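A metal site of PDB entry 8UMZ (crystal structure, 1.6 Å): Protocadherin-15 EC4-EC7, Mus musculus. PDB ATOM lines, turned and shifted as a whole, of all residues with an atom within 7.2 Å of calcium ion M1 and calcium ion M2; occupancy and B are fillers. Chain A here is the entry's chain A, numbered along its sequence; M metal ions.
Six residues have an atom within 4 Å of calcium ion M1: Glu 21, Glu 87, Asp 116, Ala 117, Asp 119 and Asp 152.
The guanidinium group of Arg 86 lies close to the side-chain carboxylate of Asp 116 (2.8 Å).
The side-chain carboxylate of Asp 200 sits close to the backbone NH of Ala 202, at 3.4 Å.
ND2 of Asn 118 sits at hydrogen-bond distance from O of His 204 (3.3 Å).
The side-chain carboxylate (OD1) of Asp 200 is in hydrogen-bond range of the backbone NH (N) of Arg 206 (2.9 Å).
N of Glu 87 is in hydrogen-bond range of OD1 of Asp 85 (3.0 Å).
OD2 of Asp 116 is in hydrogen-bond range of ND2 of Asn 156 (3.0 Å).
The side-chain carboxylate (OD2) of Asp 116 sits at hydrogen-bond distance from the backbone NH (N) of Ala 153 (3.0 Å).
The backbone NH of Glu 21 sits at hydrogen-bond distance from the backbone carbonyl oxygen of Met 115.
Calcium ion M2 is bound by OD2 of Asp 152 (2.3 Å), O of Asn 156 (2.3 Å), OD1 of Asn 118 (2.4 Å), O of Asn 120 (2.4 Å), OD2 of Asp 200 (2.4 Å), OD2 of Asp 150 (2.4 Å) and OD1 of Asp 150 (2.6 Å).
Calcium ion M2 has seven donor atoms within binding distance.
Of the 27 residues printed, 6 come within 4 Å of calcium ion M2.
Along chain A the residues within 4 Å of calcium ion M2 span positions 118 to 200.
OE2 of Glu 21 binds calcium ion M1.
OD1 of Asp 119 binds calcium ion M1.
Calcium ion M1 is bound by OD1 of Asp 116.
OD1 of Asp 152 is bound to calcium ion M1, 2.3 Å away.
Calcium ion M1 is bound by the backbone carbonyl oxygen (O) of Ala 117.
Calcium ion M1 is bound by OE2 of Glu 87 (2.6 Å).
OE1 of Glu 87 binds calcium ion M1, 2.9 Å away.
Calcium ion M1 has seven donor atoms within binding distance.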
ATOM      1  N   GLU A  21       5.225   4.698  10.873  1.00  0.00           N
ATOM      2  CA  GLU A  21       5.003   4.060   9.587  1.00  0.00           C
ATOM      3  C   GLU A  21       5.861   4.710   8.481  1.00  0.00           C
ATOM      4  O   GLU A  21       6.151   4.090   7.472  1.00  0.00           O
ATOM      5  CB  GLU A  21       3.542   4.097   9.115  1.00  0.00           C
ATOM      6  CG  GLU A  21       2.928   5.499   8.939  1.00  0.00           C
ATOM      7  CD  GLU A  21       1.464   5.369   8.586  1.00  0.00           C
ATOM      8  OE1 GLU A  21       1.145   4.496   7.840  1.00  0.00           O
ATOM      9  OE2 GLU A  21       0.606   6.248   9.012  1.00  0.00           O
ATOM     10  N   ASP A  85       2.659   0.185   6.947  1.00  0.00           N
ATOM     11  CA  ASP A  85       1.552   1.094   6.695  1.00  0.00           C
ATOM     12  C   ASP A  85       0.512   0.896   7.772  1.00  0.00           C
ATOM     13  O   ASP A  85      -0.122  -0.145   7.829  1.00  0.00           O
ATOM     14  CB  ASP A  85       1.030   0.838   5.277  1.00  0.00           C
ATOM     15  CG  ASP A  85      -0.207   1.664   4.938  1.00  0.00           C
ATOM     16  OD1 ASP A  85      -0.456   2.635   5.628  1.00  0.00           O
ATOM     17  OD2 ASP A  85      -0.878   1.332   4.003  1.00  0.00           O
ATOM     18  N   ARG A  86       0.210   1.971   8.533  1.00  0.00           N
ATOM     19  CA  ARG A  86      -0.661   1.840   9.658  1.00  0.00           C
ATOM     20  C   ARG A  86      -2.076   1.637   9.121  1.00  0.00           C
ATOM     21  O   ARG A  86      -2.853   0.937   9.741  1.00  0.00           O
ATOM     22  CB  ARG A  86      -0.502   3.044  10.584  1.00  0.00           C
ATOM     23  CG  ARG A  86      -1.245   2.844  11.896  1.00  0.00           C
ATOM     24  CD  ARG A  86      -1.682   4.192  12.413  1.00  0.00           C
ATOM     25  NE  ARG A  86      -2.701   4.779  11.558  1.00  0.00           N
ATOM     26  CZ  ARG A  86      -3.973   4.399  11.485  1.00  0.00           C
ATOM     27  NH1 ARG A  86      -4.444   3.421  12.236  1.00  0.00           N
ATOM     28  NH2 ARG A  86      -4.787   5.041  10.663  1.00  0.00           N
ATOM     29  N   GLU A  87      -2.356   2.167   7.914  1.00  0.00           N
ATOM     30  CA  GLU A  87      -3.709   2.078   7.387  1.00  0.00           C
ATOM     31  C   GLU A  87      -3.987   0.667   6.831  1.00  0.00           C
ATOM     32  O   GLU A  87      -5.142   0.311   6.608  1.00  0.00           O
ATOM     33  CB  GLU A  87      -3.911   3.113   6.282  1.00  0.00           C
ATOM     34  CG  GLU A  87      -4.157   4.526   6.801  1.00  0.00           C
ATOM     35  CD  GLU A  87      -2.983   5.240   7.437  1.00  0.00           C
ATOM     36  OE1 GLU A  87      -1.953   5.394   6.765  1.00  0.00           O
ATOM     37  OE2 GLU A  87      -3.126   5.700   8.614  1.00  0.00           O
ATOM     38  N   MET A 115       3.111   3.339  14.662  1.00  0.00           N
ATOM     39  CA  MET A 115       2.579   4.647  15.025  1.00  0.00           C
ATOM     40  C   MET A 115       2.140   5.382  13.767  1.00  0.00           C
ATOM     41  O   MET A 115       2.676   5.174  12.683  1.00  0.00           O
ATOM     42  CB  MET A 115       3.574   5.508  15.798  1.00  0.00           C
ATOM     43  CG  MET A 115       4.159   4.868  17.050  1.00  0.00           C
ATOM     44  SD  MET A 115       2.915   4.393  18.262  1.00  0.00           S
ATOM     45  CE  MET A 115       2.468   6.012  18.904  1.00  0.00           C
ATOM     46  N   ASP A 116       1.115   6.226  13.909  1.00  0.00           N
ATOM     47  CA  ASP A 116       0.575   6.925  12.762  1.00  0.00           C
ATOM     48  C   ASP A 116       1.400   8.147  12.428  1.00  0.00           C
ATOM     49  O   ASP A 116       1.776   8.977  13.267  1.00  0.00           O
ATOM     50  CB  ASP A 116      -0.871   7.306  13.070  1.00  0.00           C
ATOM     51  CG  ASP A 116      -1.577   7.897  11.869  1.00  0.00           C
ATOM     52  OD1 ASP A 116      -1.559   7.274  10.824  1.00  0.00           O
ATOM     53  OD2 ASP A 116      -2.201   8.996  12.049  1.00  0.00           O
ATOM     54  N   ALA A 117       1.655   8.288  11.135  1.00  0.00           N
ATOM     55  CA  ALA A 117       2.160   9.506  10.563  1.00  0.00           C
ATOM     56  C   ALA A 117       0.954  10.184   9.899  1.00  0.00           C
ATOM     57  O   ALA A 117       0.038   9.511   9.438  1.00  0.00           O
ATOM     58  CB  ALA A 117       3.209   9.190   9.524  1.00  0.00           C
ATOM     59  N   ASN A 118       0.975  11.513   9.844  1.00  0.00           N
ATOM     60  CA  ASN A 118       0.012  12.212   9.007  1.00  0.00           C
ATOM     61  C   ASN A 118       0.442  12.183   7.547  1.00  0.00           C
ATOM     62  O   ASN A 118       0.844  13.228   7.014  1.00  0.00           O
ATOM     63  CB  ASN A 118      -0.217  13.645   9.481  1.00  0.00           C
ATOM     64  CG  ASN A 118      -1.398  14.184   8.736  1.00  0.00           C
ATOM     65  OD1 ASN A 118      -2.327  13.432   8.461  1.00  0.00           O
ATOM     66  ND2 ASN A 118      -1.287  15.435   8.298  1.00  0.00           N
ATOM     67  N   ASP A 119       0.308  11.014   6.909  1.00  0.00           N
ATOM     68  CA  ASP A 119       0.852  10.691   5.586  1.00  0.00           C
ATOM     69  C   ASP A 119      -0.219  10.711   4.494  1.00  0.00           C
ATOM     70  O   ASP A 119       0.021  10.394   3.316  1.00  0.00           O
ATOM     71  CB  ASP A 119       1.685   9.391   5.614  1.00  0.00           C
ATOM     72  CG  ASP A 119       0.981   8.102   6.014  1.00  0.00           C
ATOM     73  OD1 ASP A 119      -0.085   8.195   6.643  1.00  0.00           O
ATOM     74  OD2 ASP A 119       1.464   6.952   5.630  1.00  0.00           O
ATOM     75  N   ASN A 120      -1.434  11.134   4.869  1.00  0.00           N
ATOM     76  CA  ASN A 120      -2.542  11.180   3.934  1.00  0.00           C
ATOM     77  C   ASN A 120      -3.163  12.576   4.020  1.00  0.00           C
ATOM     78  O   ASN A 120      -3.319  13.123   5.112  1.00  0.00           O
ATOM     79  CB  ASN A 120      -3.596  10.091   4.130  1.00  0.00           C
ATOM     80  CG  ASN A 120      -3.034   8.713   3.852  1.00  0.00           C
ATOM     81  OD1 ASN A 120      -2.530   8.064   4.756  1.00  0.00           O
ATOM     82  ND2 ASN A 120      -3.237   8.240   2.642  1.00  0.00           N
ATOM     83  N   ALA A 121      -3.495  13.123   2.857  1.00  0.00           N
ATOM     84  CA  ALA A 121      -4.359  14.282   2.787  1.00  0.00           C
ATOM     85  C   ALA A 121      -5.810  13.821   2.727  1.00  0.00           C
ATOM     86  O   ALA A 121      -6.109  12.731   2.277  1.00  0.00           O
ATOM     87  CB  ALA A 121      -3.985  15.133   1.586  1.00  0.00           C
ATOM     88  N   PRO A 122      -6.802  14.676   3.085  1.00  0.00           N
ATOM     89  CA  PRO A 122      -8.193  14.339   2.838  1.00  0.00           C
ATOM     90  C   PRO A 122      -8.399  14.079   1.341  1.00  0.00           C
ATOM     91  O   PRO A 122      -7.804  14.733   0.484  1.00  0.00           O
ATOM     92  CB  PRO A 122      -8.914  15.625   3.312  1.00  0.00           C
ATOM     93  CG  PRO A 122      -8.041  16.165   4.375  1.00  0.00           C
ATOM     94  CD  PRO A 122      -6.657  15.956   3.809  1.00  0.00           C
ATOM     95  N   ASP A 150     -10.333  11.082   5.369  1.00  0.00           N
ATOM     96  CA  ASP A 150      -8.900  10.996   5.572  1.00  0.00           C
ATOM     97  C   ASP A 150      -8.674   9.750   6.396  1.00  0.00           C
ATOM     98  O   ASP A 150      -9.188   9.651   7.517  1.00  0.00           O
ATOM     99  CB  ASP A 150      -8.444  12.244   6.324  1.00  0.00           C
ATOM    100  CG  ASP A 150      -6.943  12.432   6.477  1.00  0.00           C
ATOM    101  OD1 ASP A 150      -6.228  11.442   6.820  1.00  0.00           O
ATOM    102  OD2 ASP A 150      -6.488  13.541   6.264  1.00  0.00           O
ATOM    103  N   PRO A 151      -7.878   8.787   5.884  1.00  0.00           N
ATOM    104  CA  PRO A 151      -7.755   7.477   6.534  1.00  0.00           C
ATOM    105  C   PRO A 151      -6.801   7.495   7.743  1.00  0.00           C
ATOM    106  O   PRO A 151      -6.700   6.434   8.414  1.00  0.00           O
ATOM    107  CB  PRO A 151      -7.267   6.601   5.357  1.00  0.00           C
ATOM    108  CG  PRO A 151      -6.369   7.534   4.580  1.00  0.00           C
ATOM    109  CD  PRO A 151      -7.016   8.912   4.707  1.00  0.00           C
ATOM    110  N   ASP A 152      -6.072   8.611   8.019  1.00  0.00           N
ATOM    111  CA  ASP A 152      -5.155   8.654   9.154  1.00  0.00           C
ATOM    112  C   ASP A 152      -5.905   8.620  10.481  1.00  0.00           C
ATOM    113  O   ASP A 152      -7.129   8.658  10.501  1.00  0.00           O
ATOM    114  CB  ASP A 152      -4.189   9.835   9.135  1.00  0.00           C
ATOM    115  CG  ASP A 152      -3.360   9.945   7.877  1.00  0.00           C
ATOM    116  OD1 ASP A 152      -2.687   8.979   7.563  1.00  0.00           O
ATOM    117  OD2 ASP A 152      -3.250  11.063   7.345  1.00  0.00           O
ATOM    118  N   ALA A 153      -5.149   8.519  11.580  1.00  0.00           N
ATOM    119  CA  ALA A 153      -5.696   8.298  12.904  1.00  0.00           C
ATOM    120  C   ALA A 153      -5.906   9.602  13.655  1.00  0.00           C
ATOM    121  O   ALA A 153      -5.091  10.524  13.631  1.00  0.00           O
ATOM    122  CB  ALA A 153      -4.740   7.431  13.706  1.00  0.00           C
ATOM    123  N   ILE A 155      -6.616  12.953  15.120  1.00  0.00           N
ATOM    124  CA  ILE A 155      -6.717  14.325  14.575  1.00  0.00           C
ATOM    125  C   ILE A 155      -6.160  14.329  13.158  1.00  0.00           C
ATOM    126  O   ILE A 155      -6.598  15.089  12.277  1.00  0.00           O
ATOM    127  CB  ILE A 155      -5.980  15.364  15.411  1.00  0.00           C
ATOM    128  CG1 ILE A 155      -4.457  15.055  15.495  1.00  0.00           C
ATOM    129  CG2 ILE A 155      -6.597  15.587  16.755  1.00  0.00           C
ATOM    130  CD1 ILE A 155      -3.736  15.964  16.472  1.00  0.00           C
ATOM    131  N   ASN A 156      -5.249  13.385  12.865  1.00  0.00           N
ATOM    132  CA  ASN A 156      -4.653  13.328  11.540  1.00  0.00           C
ATOM    133  C   ASN A 156      -5.689  12.916  10.480  1.00  0.00           C
ATOM    134  O   ASN A 156      -5.411  13.123   9.316  1.00  0.00           O
ATOM    135  CB  ASN A 156      -3.410  12.409  11.518  1.00  0.00           C
ATOM    136  CG  ASN A 156      -2.307  12.787  12.471  1.00  0.00           C
ATOM    137  OD1 ASN A 156      -2.154  13.956  12.865  1.00  0.00           O
ATOM    138  ND2 ASN A 156      -1.489  11.791  12.859  1.00  0.00           N
ATOM    139  N   GLY A 157      -6.825  12.316  10.884  1.00  0.00           N
ATOM    140  CA  GLY A 157      -7.881  11.860  10.001  1.00  0.00           C
ATOM    141  C   GLY A 157      -9.165  12.689  10.145  1.00  0.00           C
ATOM    142  O   GLY A 157     -10.105  12.388   9.438  1.00  0.00           O
ATOM    143  N   GLN A 158      -9.164  13.741  10.979  1.00  0.00           N
ATOM    144  CA  GLN A 158     -10.343  14.608  11.120  1.00  0.00           C
ATOM    145  C   GLN A 158     -10.283  15.761  10.136  1.00  0.00           C
ATOM    146  O   GLN A 158      -9.249  16.387   9.925  1.00  0.00           O
ATOM    147  CB  GLN A 158     -10.517  15.079  12.548  1.00  0.00           C
ATOM    148  CG  GLN A 158     -10.912  13.948  13.476  1.00  0.00           C
ATOM    149  CD  GLN A 158     -10.751  14.388  14.911  1.00  0.00           C
ATOM    150  OE1 GLN A 158     -10.668  15.576  15.270  1.00  0.00           O
ATOM    151  NE2 GLN A 158     -10.608  13.406  15.772  1.00  0.00           N
ATOM    152  N   THR A 199      -9.010  20.207   5.115  1.00  0.00           N
ATOM    153  CA  THR A 199      -7.754  20.234   5.891  1.00  0.00           C
ATOM    154  C   THR A 199      -7.916  19.283   7.075  1.00  0.00           C
ATOM    155  O   THR A 199      -8.944  19.237   7.734  1.00  0.00           O
ATOM    156  CB  THR A 199      -7.465  21.630   6.415  1.00  0.00           C
ATOM    157  OG1 THR A 199      -7.421  22.583   5.329  1.00  0.00           O
ATOM    158  CG2 THR A 199      -6.176  21.721   7.209  1.00  0.00           C
ATOM    159  N   ASP A 200      -6.919  18.423   7.321  1.00  0.00           N
ATOM    160  CA  ASP A 200      -6.984  17.610   8.526  1.00  0.00           C
ATOM    161  C   ASP A 200      -6.578  18.387   9.778  1.00  0.00           C
ATOM    162  O   ASP A 200      -6.158  19.541   9.727  1.00  0.00           O
ATOM    163  CB  ASP A 200      -6.232  16.296   8.297  1.00  0.00           C
ATOM    164  CG  ASP A 200      -4.752  16.416   7.973  1.00  0.00           C
ATOM    165  OD1 ASP A 200      -4.168  17.331   8.492  1.00  0.00           O
ATOM    166  OD2 ASP A 200      -4.206  15.496   7.203  1.00  0.00           O
ATOM    167  N   GLY A 201      -6.732  17.703  10.935  1.00  0.00           N
ATOM    168  CA  GLY A 201      -6.447  18.241  12.249  1.00  0.00           C
ATOM    169  C   GLY A 201      -5.019  18.014  12.748  1.00  0.00           C
ATOM    170  O   GLY A 201      -4.758  18.329  13.892  1.00  0.00           O
ATOM    171  N   ALA A 202      -4.074  17.617  11.915  1.00  0.00           N
ATOM    172  CA  ALA A 202      -2.735  17.306  12.384  1.00  0.00           C
ATOM    173  C   ALA A 202      -1.995  18.537  12.886  1.00  0.00           C
ATOM    174  O   ALA A 202      -2.245  19.671  12.457  1.00  0.00           O
ATOM    175  CB  ALA A 202      -1.987  16.665  11.279  1.00  0.00           C
ATOM    176  N   HIS A 204       0.928  19.060  11.945  1.00  0.00           N
ATOM    177  CA  HIS A 204       1.520  19.467  10.681  1.00  0.00           C
ATOM    178  C   HIS A 204       0.445  19.183   9.634  1.00  0.00           C
ATOM    179  O   HIS A 204       0.421  18.087   9.093  1.00  0.00           O
ATOM    180  CB  HIS A 204       2.831  18.694  10.469  1.00  0.00           C
ATOM    181  CG  HIS A 204       3.846  18.872  11.555  1.00  0.00           C
ATOM    182  ND1 HIS A 204       4.335  17.816  12.306  1.00  0.00           N
ATOM    183  CD2 HIS A 204       4.486  19.977  12.000  1.00  0.00           C
ATOM    184  CE1 HIS A 204       5.234  18.299  13.175  1.00  0.00           C
ATOM    185  NE2 HIS A 204       5.358  19.587  12.983  1.00  0.00           N
ATOM    186  N   PRO A 205      -0.557  20.073   9.436  1.00  0.00           N
ATOM    187  CA  PRO A 205      -1.757  19.689   8.672  1.00  0.00           C
ATOM    188  C   PRO A 205      -1.470  19.376   7.221  1.00  0.00           C
ATOM    189  O   PRO A 205      -0.518  19.913   6.644  1.00  0.00           O
ATOM    190  CB  PRO A 205      -2.657  20.919   8.827  1.00  0.00           C
ATOM    191  CG  PRO A 205      -1.679  22.033   9.092  1.00  0.00           C
ATOM    192  CD  PRO A 205      -0.715  21.381  10.066  1.00  0.00           C
ATOM    193  N   ARG A 206      -2.313  18.542   6.619  1.00  0.00           N
ATOM    194  CA  ARG A 206      -2.317  18.335   5.163  1.00  0.00           C
ATOM    195  C   ARG A 206      -3.690  18.777   4.653  1.00  0.00           C
ATOM    196  O   ARG A 206      -4.664  18.738   5.413  1.00  0.00           O
ATOM    197  CB  ARG A 206      -2.015  16.905   4.754  1.00  0.00           C
ATOM    198  CG  ARG A 206      -0.565  16.476   4.938  1.00  0.00           C
ATOM    199  CD  ARG A 206      -0.385  15.078   4.397  1.00  0.00           C
ATOM    200  NE  ARG A 206       1.001  14.576   4.463  1.00  0.00           N
ATOM    201  CZ  ARG A 206       1.947  14.886   3.563  1.00  0.00           C
ATOM    202  NH1 ARG A 206       1.678  15.713   2.569  1.00  0.00           N
ATOM    203  NH2 ARG A 206       3.187  14.412   3.680  1.00  0.00           N
HETATM  204 CA    CA M   1      -1.187   7.493   8.544  1.00  0.00          CA
HETATM  205 CA    CA M   2      -4.324  13.117   7.254  1.00  0.00          CA
